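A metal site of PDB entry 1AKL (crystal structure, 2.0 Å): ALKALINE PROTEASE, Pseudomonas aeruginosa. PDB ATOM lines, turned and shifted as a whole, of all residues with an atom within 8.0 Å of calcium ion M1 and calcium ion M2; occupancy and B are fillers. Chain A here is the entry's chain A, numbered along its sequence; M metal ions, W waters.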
ATOM      1  N   THR A 252      -4.506 -23.942  22.168  1.00  0.00           N
ATOM      2  CA  THR A 252      -5.067 -22.833  21.400  1.00  0.00           C
ATOM      3  C   THR A 252      -6.555 -22.617  21.442  1.00  0.00           C
ATOM      4  O   THR A 252      -7.333 -23.485  21.069  1.00  0.00           O
ATOM      5  CB  THR A 252      -4.630 -22.916  19.955  1.00  0.00           C
ATOM      6  OG1 THR A 252      -3.202 -22.907  19.915  1.00  0.00           O
ATOM      7  CG2 THR A 252      -5.154 -21.740  19.156  1.00  0.00           C
ATOM      8  N   ARG A 253      -6.949 -21.412  21.824  1.00  0.00           N
ATOM      9  CA  ARG A 253      -8.343 -21.026  21.902  1.00  0.00           C
ATOM     10  C   ARG A 253      -9.208 -22.034  22.677  1.00  0.00           C
ATOM     11  O   ARG A 253     -10.276 -22.441  22.199  1.00  0.00           O
ATOM     12  CB  ARG A 253      -8.884 -20.802  20.487  1.00  0.00           C
ATOM     13  CG  ARG A 253      -8.259 -19.592  19.793  1.00  0.00           C
ATOM     14  CD  ARG A 253      -8.797 -19.321  18.381  1.00  0.00           C
ATOM     15  NE  ARG A 253      -8.227 -20.186  17.342  1.00  0.00           N
ATOM     16  CZ  ARG A 253      -7.044 -19.997  16.747  1.00  0.00           C
ATOM     17  NH1 ARG A 253      -6.262 -18.983  17.074  1.00  0.00           N
ATOM     18  NH2 ARG A 253      -6.654 -20.815  15.785  1.00  0.00           N
ATOM     19  N   THR A 254      -8.778 -22.388  23.891  1.00  0.00           N
ATOM     20  CA  THR A 254      -9.538 -23.340  24.711  1.00  0.00           C
ATOM     21  C   THR A 254     -10.797 -22.768  25.335  1.00  0.00           C
ATOM     22  O   THR A 254     -11.539 -23.487  26.002  1.00  0.00           O
ATOM     23  CB  THR A 254      -8.679 -23.998  25.830  1.00  0.00           C
ATOM     24  OG1 THR A 254      -8.228 -23.009  26.761  1.00  0.00           O
ATOM     25  CG2 THR A 254      -7.481 -24.717  25.236  1.00  0.00           C
ATOM     26  N   GLY A 255     -11.051 -21.479  25.131  1.00  0.00           N
ATOM     27  CA  GLY A 255     -12.254 -20.891  25.686  1.00  0.00           C
ATOM     28  C   GLY A 255     -13.392 -20.943  24.686  1.00  0.00           C
ATOM     29  O   GLY A 255     -13.280 -21.586  23.631  1.00  0.00           O
ATOM     30  N   ASP A 256     -14.490 -20.263  25.005  1.00  0.00           N
ATOM     31  CA  ASP A 256     -15.648 -20.229  24.120  1.00  0.00           C
ATOM     32  C   ASP A 256     -15.330 -19.166  23.088  1.00  0.00           C
ATOM     33  O   ASP A 256     -15.439 -17.962  23.357  1.00  0.00           O
ATOM     34  CB  ASP A 256     -16.906 -19.898  24.925  1.00  0.00           C
ATOM     35  CG  ASP A 256     -17.101 -20.811  26.103  1.00  0.00           C
ATOM     36  OD1 ASP A 256     -16.564 -21.949  26.092  1.00  0.00           O
ATOM     37  OD2 ASP A 256     -17.759 -20.396  27.065  1.00  0.00           O
ATOM     38  N   THR A 257     -14.962 -19.638  21.908  1.00  0.00           N
ATOM     39  CA  THR A 257     -14.514 -18.789  20.805  1.00  0.00           C
ATOM     40  C   THR A 257     -15.531 -18.528  19.692  1.00  0.00           C
ATOM     41  O   THR A 257     -16.244 -19.436  19.265  1.00  0.00           O
ATOM     42  CB  THR A 257     -13.255 -19.397  20.171  1.00  0.00           C
ATOM     43  OG1 THR A 257     -12.558 -20.185  21.157  1.00  0.00           O
ATOM     44  CG2 THR A 257     -12.355 -18.326  19.720  1.00  0.00           C
ATOM     45  N   VAL A 258     -15.571 -17.290  19.208  1.00  0.00           N
ATOM     46  CA  VAL A 258     -16.468 -16.906  18.137  1.00  0.00           C
ATOM     47  C   VAL A 258     -15.614 -16.569  16.910  1.00  0.00           C
ATOM     48  O   VAL A 258     -14.645 -15.816  17.017  1.00  0.00           O
ATOM     49  CB  VAL A 258     -17.327 -15.672  18.523  1.00  0.00           C
ATOM     50  CG1 VAL A 258     -18.267 -15.292  17.386  1.00  0.00           C
ATOM     51  CG2 VAL A 258     -18.146 -15.944  19.784  1.00  0.00           C
ATOM     52  N   TYR A 259     -15.951 -17.153  15.773  1.00  0.00           N
ATOM     53  CA  TYR A 259     -15.242 -16.885  14.530  1.00  0.00           C
ATOM     54  C   TYR A 259     -16.184 -16.155  13.608  1.00  0.00           C
ATOM     55  O   TYR A 259     -17.362 -16.493  13.559  1.00  0.00           O
ATOM     56  CB  TYR A 259     -14.818 -18.182  13.899  1.00  0.00           C
ATOM     57  CG  TYR A 259     -13.917 -18.977  14.774  1.00  0.00           C
ATOM     58  CD1 TYR A 259     -14.427 -19.860  15.722  1.00  0.00           C
ATOM     59  CD2 TYR A 259     -12.542 -18.889  14.632  1.00  0.00           C
ATOM     60  CE1 TYR A 259     -13.590 -20.625  16.522  1.00  0.00           C
ATOM     61  CE2 TYR A 259     -11.691 -19.652  15.416  1.00  0.00           C
ATOM     62  CZ  TYR A 259     -12.219 -20.525  16.359  1.00  0.00           C
ATOM     63  OH  TYR A 259     -11.367 -21.290  17.118  1.00  0.00           O
ATOM     64  N   ASN A 264     -13.694 -13.066  18.923  1.00  0.00           N
ATOM     65  CA  ASN A 264     -12.898 -12.798  20.109  1.00  0.00           C
ATOM     66  C   ASN A 264     -11.544 -13.507  20.028  1.00  0.00           C
ATOM     67  O   ASN A 264     -10.865 -13.740  21.028  1.00  0.00           O
ATOM     68  CB  ASN A 264     -13.659 -13.129  21.406  1.00  0.00           C
ATOM     69  CG  ASN A 264     -14.040 -14.585  21.521  1.00  0.00           C
ATOM     70  OD1 ASN A 264     -13.940 -15.340  20.552  1.00  0.00           O
ATOM     71  ND2 ASN A 264     -14.509 -14.990  22.694  1.00  0.00           N
ATOM     72  N   THR A 265     -11.170 -13.894  18.794  1.00  0.00           N
ATOM     73  CA  THR A 265      -9.876 -14.503  18.496  1.00  0.00           C
ATOM     74  C   THR A 265      -9.142 -13.262  18.003  1.00  0.00           C
ATOM     75  O   THR A 265      -9.559 -12.653  17.012  1.00  0.00           O
ATOM     76  CB  THR A 265      -9.945 -15.497  17.276  1.00  0.00           C
ATOM     77  OG1 THR A 265     -10.254 -14.784  16.066  1.00  0.00           O
ATOM     78  CG2 THR A 265     -10.978 -16.579  17.476  1.00  0.00           C
ATOM     79  N   VAL A 283     -10.566 -23.302  10.604  1.00  0.00           N
ATOM     80  CA  VAL A 283     -10.619 -23.218  12.059  1.00  0.00           C
ATOM     81  C   VAL A 283      -9.784 -24.269  12.797  1.00  0.00           C
ATOM     82  O   VAL A 283      -9.859 -25.458  12.492  1.00  0.00           O
ATOM     83  CB  VAL A 283     -12.087 -23.332  12.548  1.00  0.00           C
ATOM     84  CG1 VAL A 283     -12.169 -23.305  14.061  1.00  0.00           C
ATOM     85  CG2 VAL A 283     -12.910 -22.213  11.946  1.00  0.00           C
ATOM     86  N   TRP A 284      -8.917 -23.803  13.686  1.00  0.00           N
ATOM     87  CA  TRP A 284      -8.162 -24.709  14.527  1.00  0.00           C
ATOM     88  C   TRP A 284      -8.535 -24.233  15.920  1.00  0.00           C
ATOM     89  O   TRP A 284      -8.327 -23.060  16.255  1.00  0.00           O
ATOM     90  CB  TRP A 284      -6.649 -24.622  14.342  1.00  0.00           C
ATOM     91  CG  TRP A 284      -5.976 -25.407  15.430  1.00  0.00           C
ATOM     92  CD1 TRP A 284      -5.299 -24.899  16.491  1.00  0.00           C
ATOM     93  CD2 TRP A 284      -6.068 -26.821  15.650  1.00  0.00           C
ATOM     94  NE1 TRP A 284      -4.978 -25.899  17.374  1.00  0.00           N
ATOM     95  CE2 TRP A 284      -5.440 -27.094  16.876  1.00  0.00           C
ATOM     96  CE3 TRP A 284      -6.642 -27.888  14.932  1.00  0.00           C
ATOM     97  CZ2 TRP A 284      -5.355 -28.387  17.420  1.00  0.00           C
ATOM     98  CZ3 TRP A 284      -6.563 -29.180  15.464  1.00  0.00           C
ATOM     99  CH2 TRP A 284      -5.921 -29.420  16.701  1.00  0.00           C
ATOM    100  N   ASP A 285      -9.101 -25.128  16.720  1.00  0.00           N
ATOM    101  CA  ASP A 285      -9.562 -24.801  18.060  1.00  0.00           C
ATOM    102  C   ASP A 285      -9.396 -26.051  18.927  1.00  0.00           C
ATOM    103  O   ASP A 285      -9.809 -27.141  18.531  1.00  0.00           O
ATOM    104  CB  ASP A 285     -11.032 -24.380  17.972  1.00  0.00           C
ATOM    105  CG  ASP A 285     -11.549 -23.749  19.229  1.00  0.00           C
ATOM    106  OD1 ASP A 285     -11.686 -24.444  20.248  1.00  0.00           O
ATOM    107  OD2 ASP A 285     -11.852 -22.537  19.216  1.00  0.00           O
ATOM    108  N   ALA A 286      -8.802 -25.882  20.102  1.00  0.00           N
ATOM    109  CA  ALA A 286      -8.543 -27.004  20.985  1.00  0.00           C
ATOM    110  C   ALA A 286      -9.529 -27.222  22.114  1.00  0.00           C
ATOM    111  O   ALA A 286      -9.330 -28.127  22.918  1.00  0.00           O
ATOM    112  CB  ALA A 286      -7.142 -26.884  21.532  1.00  0.00           C
ATOM    113  N   GLY A 287     -10.581 -26.418  22.209  1.00  0.00           N
ATOM    114  CA  GLY A 287     -11.542 -26.632  23.269  1.00  0.00           C
ATOM    115  C   GLY A 287     -12.597 -25.564  23.443  1.00  0.00           C
ATOM    116  O   GLY A 287     -12.533 -24.497  22.783  1.00  0.00           O
ATOM    117  N   GLY A 288     -13.609 -25.871  24.265  1.00  0.00           N
ATOM    118  CA  GLY A 288     -14.681 -24.937  24.542  1.00  0.00           C
ATOM    119  C   GLY A 288     -15.891 -24.947  23.633  1.00  0.00           C
ATOM    120  O   GLY A 288     -15.933 -25.661  22.615  1.00  0.00           O
ATOM    121  N   ASN A 289     -16.856 -24.111  23.981  1.00  0.00           N
ATOM    122  CA  ASN A 289     -18.111 -23.973  23.245  1.00  0.00           C
ATOM    123  C   ASN A 289     -17.913 -22.867  22.210  1.00  0.00           C
ATOM    124  O   ASN A 289     -17.911 -21.679  22.538  1.00  0.00           O
ATOM    125  CB  ASN A 289     -19.234 -23.635  24.228  1.00  0.00           C
ATOM    126  CG  ASN A 289     -20.588 -23.616  23.569  1.00  0.00           C
ATOM    127  OD1 ASN A 289     -20.976 -24.584  22.928  1.00  0.00           O
ATOM    128  ND2 ASN A 289     -21.326 -22.522  23.742  1.00  0.00           N
ATOM    129  N   ASP A 290     -17.803 -23.269  20.949  1.00  0.00           N
ATOM    130  CA  ASP A 290     -17.526 -22.341  19.849  1.00  0.00           C
ATOM    131  C   ASP A 290     -18.652 -22.062  18.901  1.00  0.00           C
ATOM    132  O   ASP A 290     -19.467 -22.925  18.630  1.00  0.00           O
ATOM    133  CB  ASP A 290     -16.315 -22.849  19.096  1.00  0.00           C
ATOM    134  CG  ASP A 290     -15.214 -23.277  20.021  1.00  0.00           C
ATOM    135  OD1 ASP A 290     -14.654 -22.415  20.705  1.00  0.00           O
ATOM    136  OD2 ASP A 290     -14.950 -24.495  20.119  1.00  0.00           O
ATOM    137  N   THR A 291     -18.614 -20.875  18.306  1.00  0.00           N
ATOM    138  CA  THR A 291     -19.647 -20.432  17.386  1.00  0.00           C
ATOM    139  C   THR A 291     -19.067 -19.830  16.136  1.00  0.00           C
ATOM    140  O   THR A 291     -18.074 -19.108  16.187  1.00  0.00           O
ATOM    141  CB  THR A 291     -20.480 -19.324  18.039  1.00  0.00           C
ATOM    142  OG1 THR A 291     -20.875 -19.733  19.357  1.00  0.00           O
ATOM    143  CG2 THR A 291     -21.706 -18.995  17.206  1.00  0.00           C
ATOM    144  N   VAL A 326     -11.309 -31.007  15.061  1.00  0.00           N
ATOM    145  CA  VAL A 326     -11.925 -29.835  15.674  1.00  0.00           C
ATOM    146  C   VAL A 326     -13.442 -29.983  15.743  1.00  0.00           C
ATOM    147  O   VAL A 326     -14.078 -30.426  14.779  1.00  0.00           O
ATOM    148  CB  VAL A 326     -11.527 -28.537  14.909  1.00  0.00           C
ATOM    149  CG1 VAL A 326     -12.278 -27.326  15.461  1.00  0.00           C
ATOM    150  CG2 VAL A 326     -10.040 -28.303  15.032  1.00  0.00           C
ATOM    151  N   THR A 327     -14.010 -29.635  16.893  1.00  0.00           N
ATOM    152  CA  THR A 327     -15.457 -29.681  17.102  1.00  0.00           C
ATOM    153  C   THR A 327     -15.994 -28.279  17.367  1.00  0.00           C
ATOM    154  O   THR A 327     -15.775 -27.712  18.447  1.00  0.00           O
ATOM    155  CB  THR A 327     -15.836 -30.571  18.301  1.00  0.00           C
ATOM    156  OG1 THR A 327     -15.290 -31.884  18.117  1.00  0.00           O
ATOM    157  CG2 THR A 327     -17.333 -30.687  18.417  1.00  0.00           C
ATOM    158  N   VAL A 328     -16.638 -27.686  16.369  1.00  0.00           N
ATOM    159  CA  VAL A 328     -17.241 -26.368  16.519  1.00  0.00           C
ATOM    160  C   VAL A 328     -18.702 -26.696  16.865  1.00  0.00           C
ATOM    161  O   VAL A 328     -19.301 -27.565  16.242  1.00  0.00           O
ATOM    162  CB  VAL A 328     -17.152 -25.561  15.221  1.00  0.00           C
ATOM    163  CG1 VAL A 328     -17.876 -24.235  15.356  1.00  0.00           C
ATOM    164  CG2 VAL A 328     -15.697 -25.327  14.870  1.00  0.00           C
ATOM    165  N   GLU A 329     -19.267 -26.017  17.855  1.00  0.00           N
ATOM    166  CA  GLU A 329     -20.605 -26.339  18.281  1.00  0.00           C
ATOM    167  C   GLU A 329     -21.780 -25.575  17.705  1.00  0.00           C
ATOM    168  O   GLU A 329     -22.828 -26.166  17.500  1.00  0.00           O
ATOM    169  CB  GLU A 329     -20.709 -26.283  19.801  1.00  0.00           C
ATOM    170  CG  GLU A 329     -19.993 -27.380  20.527  1.00  0.00           C
ATOM    171  CD  GLU A 329     -18.504 -27.173  20.606  1.00  0.00           C
ATOM    172  OE1 GLU A 329     -17.996 -26.097  20.231  1.00  0.00           O
ATOM    173  OE2 GLU A 329     -17.817 -28.101  21.071  1.00  0.00           O
ATOM    174  N   ASN A 330     -21.633 -24.280  17.454  1.00  0.00           N
ATOM    175  CA  ASN A 330     -22.763 -23.499  16.960  1.00  0.00           C
ATOM    176  C   ASN A 330     -22.479 -22.691  15.710  1.00  0.00           C
ATOM    177  O   ASN A 330     -21.335 -22.382  15.396  1.00  0.00           O
ATOM    178  CB  ASN A 330     -23.247 -22.532  18.049  1.00  0.00           C
ATOM    179  CG  ASN A 330     -23.085 -23.106  19.440  1.00  0.00           C
ATOM    180  OD1 ASN A 330     -23.599 -24.183  19.753  1.00  0.00           O
ATOM    181  ND2 ASN A 330     -22.332 -22.404  20.281  1.00  0.00           N
ATOM    182  N   ASN A 343     -23.149 -31.115  13.360  1.00  0.00           N
ATOM    183  CA  ASN A 343     -22.338 -32.316  13.422  1.00  0.00           C
ATOM    184  C   ASN A 343     -22.911 -33.247  14.464  1.00  0.00           C
ATOM    185  O   ASN A 343     -24.041 -33.039  14.916  1.00  0.00           O
ATOM    186  CB  ASN A 343     -20.877 -31.982  13.712  1.00  0.00           C
ATOM    187  CG  ASN A 343     -20.715 -31.092  14.921  1.00  0.00           C
ATOM    188  OD1 ASN A 343     -21.504 -31.158  15.860  1.00  0.00           O
ATOM    189  ND2 ASN A 343     -19.709 -30.222  14.897  1.00  0.00           N
ATOM    190  N   VAL A 345     -22.356 -33.635  17.737  1.00  0.00           N
ATOM    191  CA  VAL A 345     -22.663 -33.129  19.072  1.00  0.00           C
ATOM    192  C   VAL A 345     -23.889 -32.238  19.075  1.00  0.00           C
ATOM    193  O   VAL A 345     -24.529 -32.032  18.027  1.00  0.00           O
ATOM    194  CB  VAL A 345     -21.457 -32.396  19.703  1.00  0.00           C
ATOM    195  CG1 VAL A 345     -20.239 -33.291  19.729  1.00  0.00           C
ATOM    196  CG2 VAL A 345     -21.163 -31.111  18.960  1.00  0.00           C
HETATM  197 CA    CA M   1     -12.459 -22.428  21.659  1.00  0.00          CA
HETATM  198 CA    CA M   2     -15.631 -26.828  20.657  1.00  0.00          CA
HETATM  199  O   HOH W   1     -14.903 -28.778  21.695  1.00  0.00           O
HETATM  200  O   HOH W   2     -13.250 -26.892  20.038  1.00  0.00           O
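The guanidinium group (NE) of Arg 253 is in hydrogen-bond range of the side-chain hydroxyl (OH) of Tyr 259 (3.3 Å). The guanidinium group (NH2) of Arg 253 is in hydrogen-bond range of the backbone carbonyl oxygen (O) of Trp 284, at 2.8 Å. The backbone NH (N) of Thr 291 sits at hydrogen-bond distance from the backbone carbonyl oxygen (O) of Thr 257. O of Asp 290 is in hydrogen-bond range of N of Asn 330, at 2.8 Å. OH of Tyr 259 lies close to OD2 of Asp 285, 2.5 Å away.
Six residues have an atom within 4 Å of calcium ion M1: Arg 253, Gly 255, Thr 257, Asp 285, Gly 287 and Asp 290. The nearest printed residue that does not touch calcium ion M1 is Thr 254 (4.05 Å).
Four residues have an atom within 4 Å of calcium ion M2: Gly 288, Asp 290, Thr 327 and Glu 329. The nearest printed residue that does not touch calcium ion M2 is Gly 287 (4.3 Å).
O of Arg 253 binds calcium ion M1 (2.2 Å). Calcium ion M1 is bound by O of Gly 255. Calcium ion M1 is bound by OG1 of Thr 257 (2.3 Å). O of Gly 287 is bound to calcium ion M1 (2.4 Å). OD1 of Asp 290 is bound to calcium ion M1 (2.4 Å). OD2 of Asp 285 is bound to calcium ion M1. OD1 of Asp 285 is bound to calcium ion M1.
Calcium ion M2 is bound by the backbone carbonyl oxygen (O) of Gly 288, water W1, the backbone carbonyl oxygen (O) of Thr 327, water W2, the side-chain carboxylate (OD2) of Asp 290, the side-chain carboxylate (OE1) of Glu 329 and the side-chain carboxylate (OE2) of Glu 329. Calcium ion M2 has seven donor atoms within binding distance.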
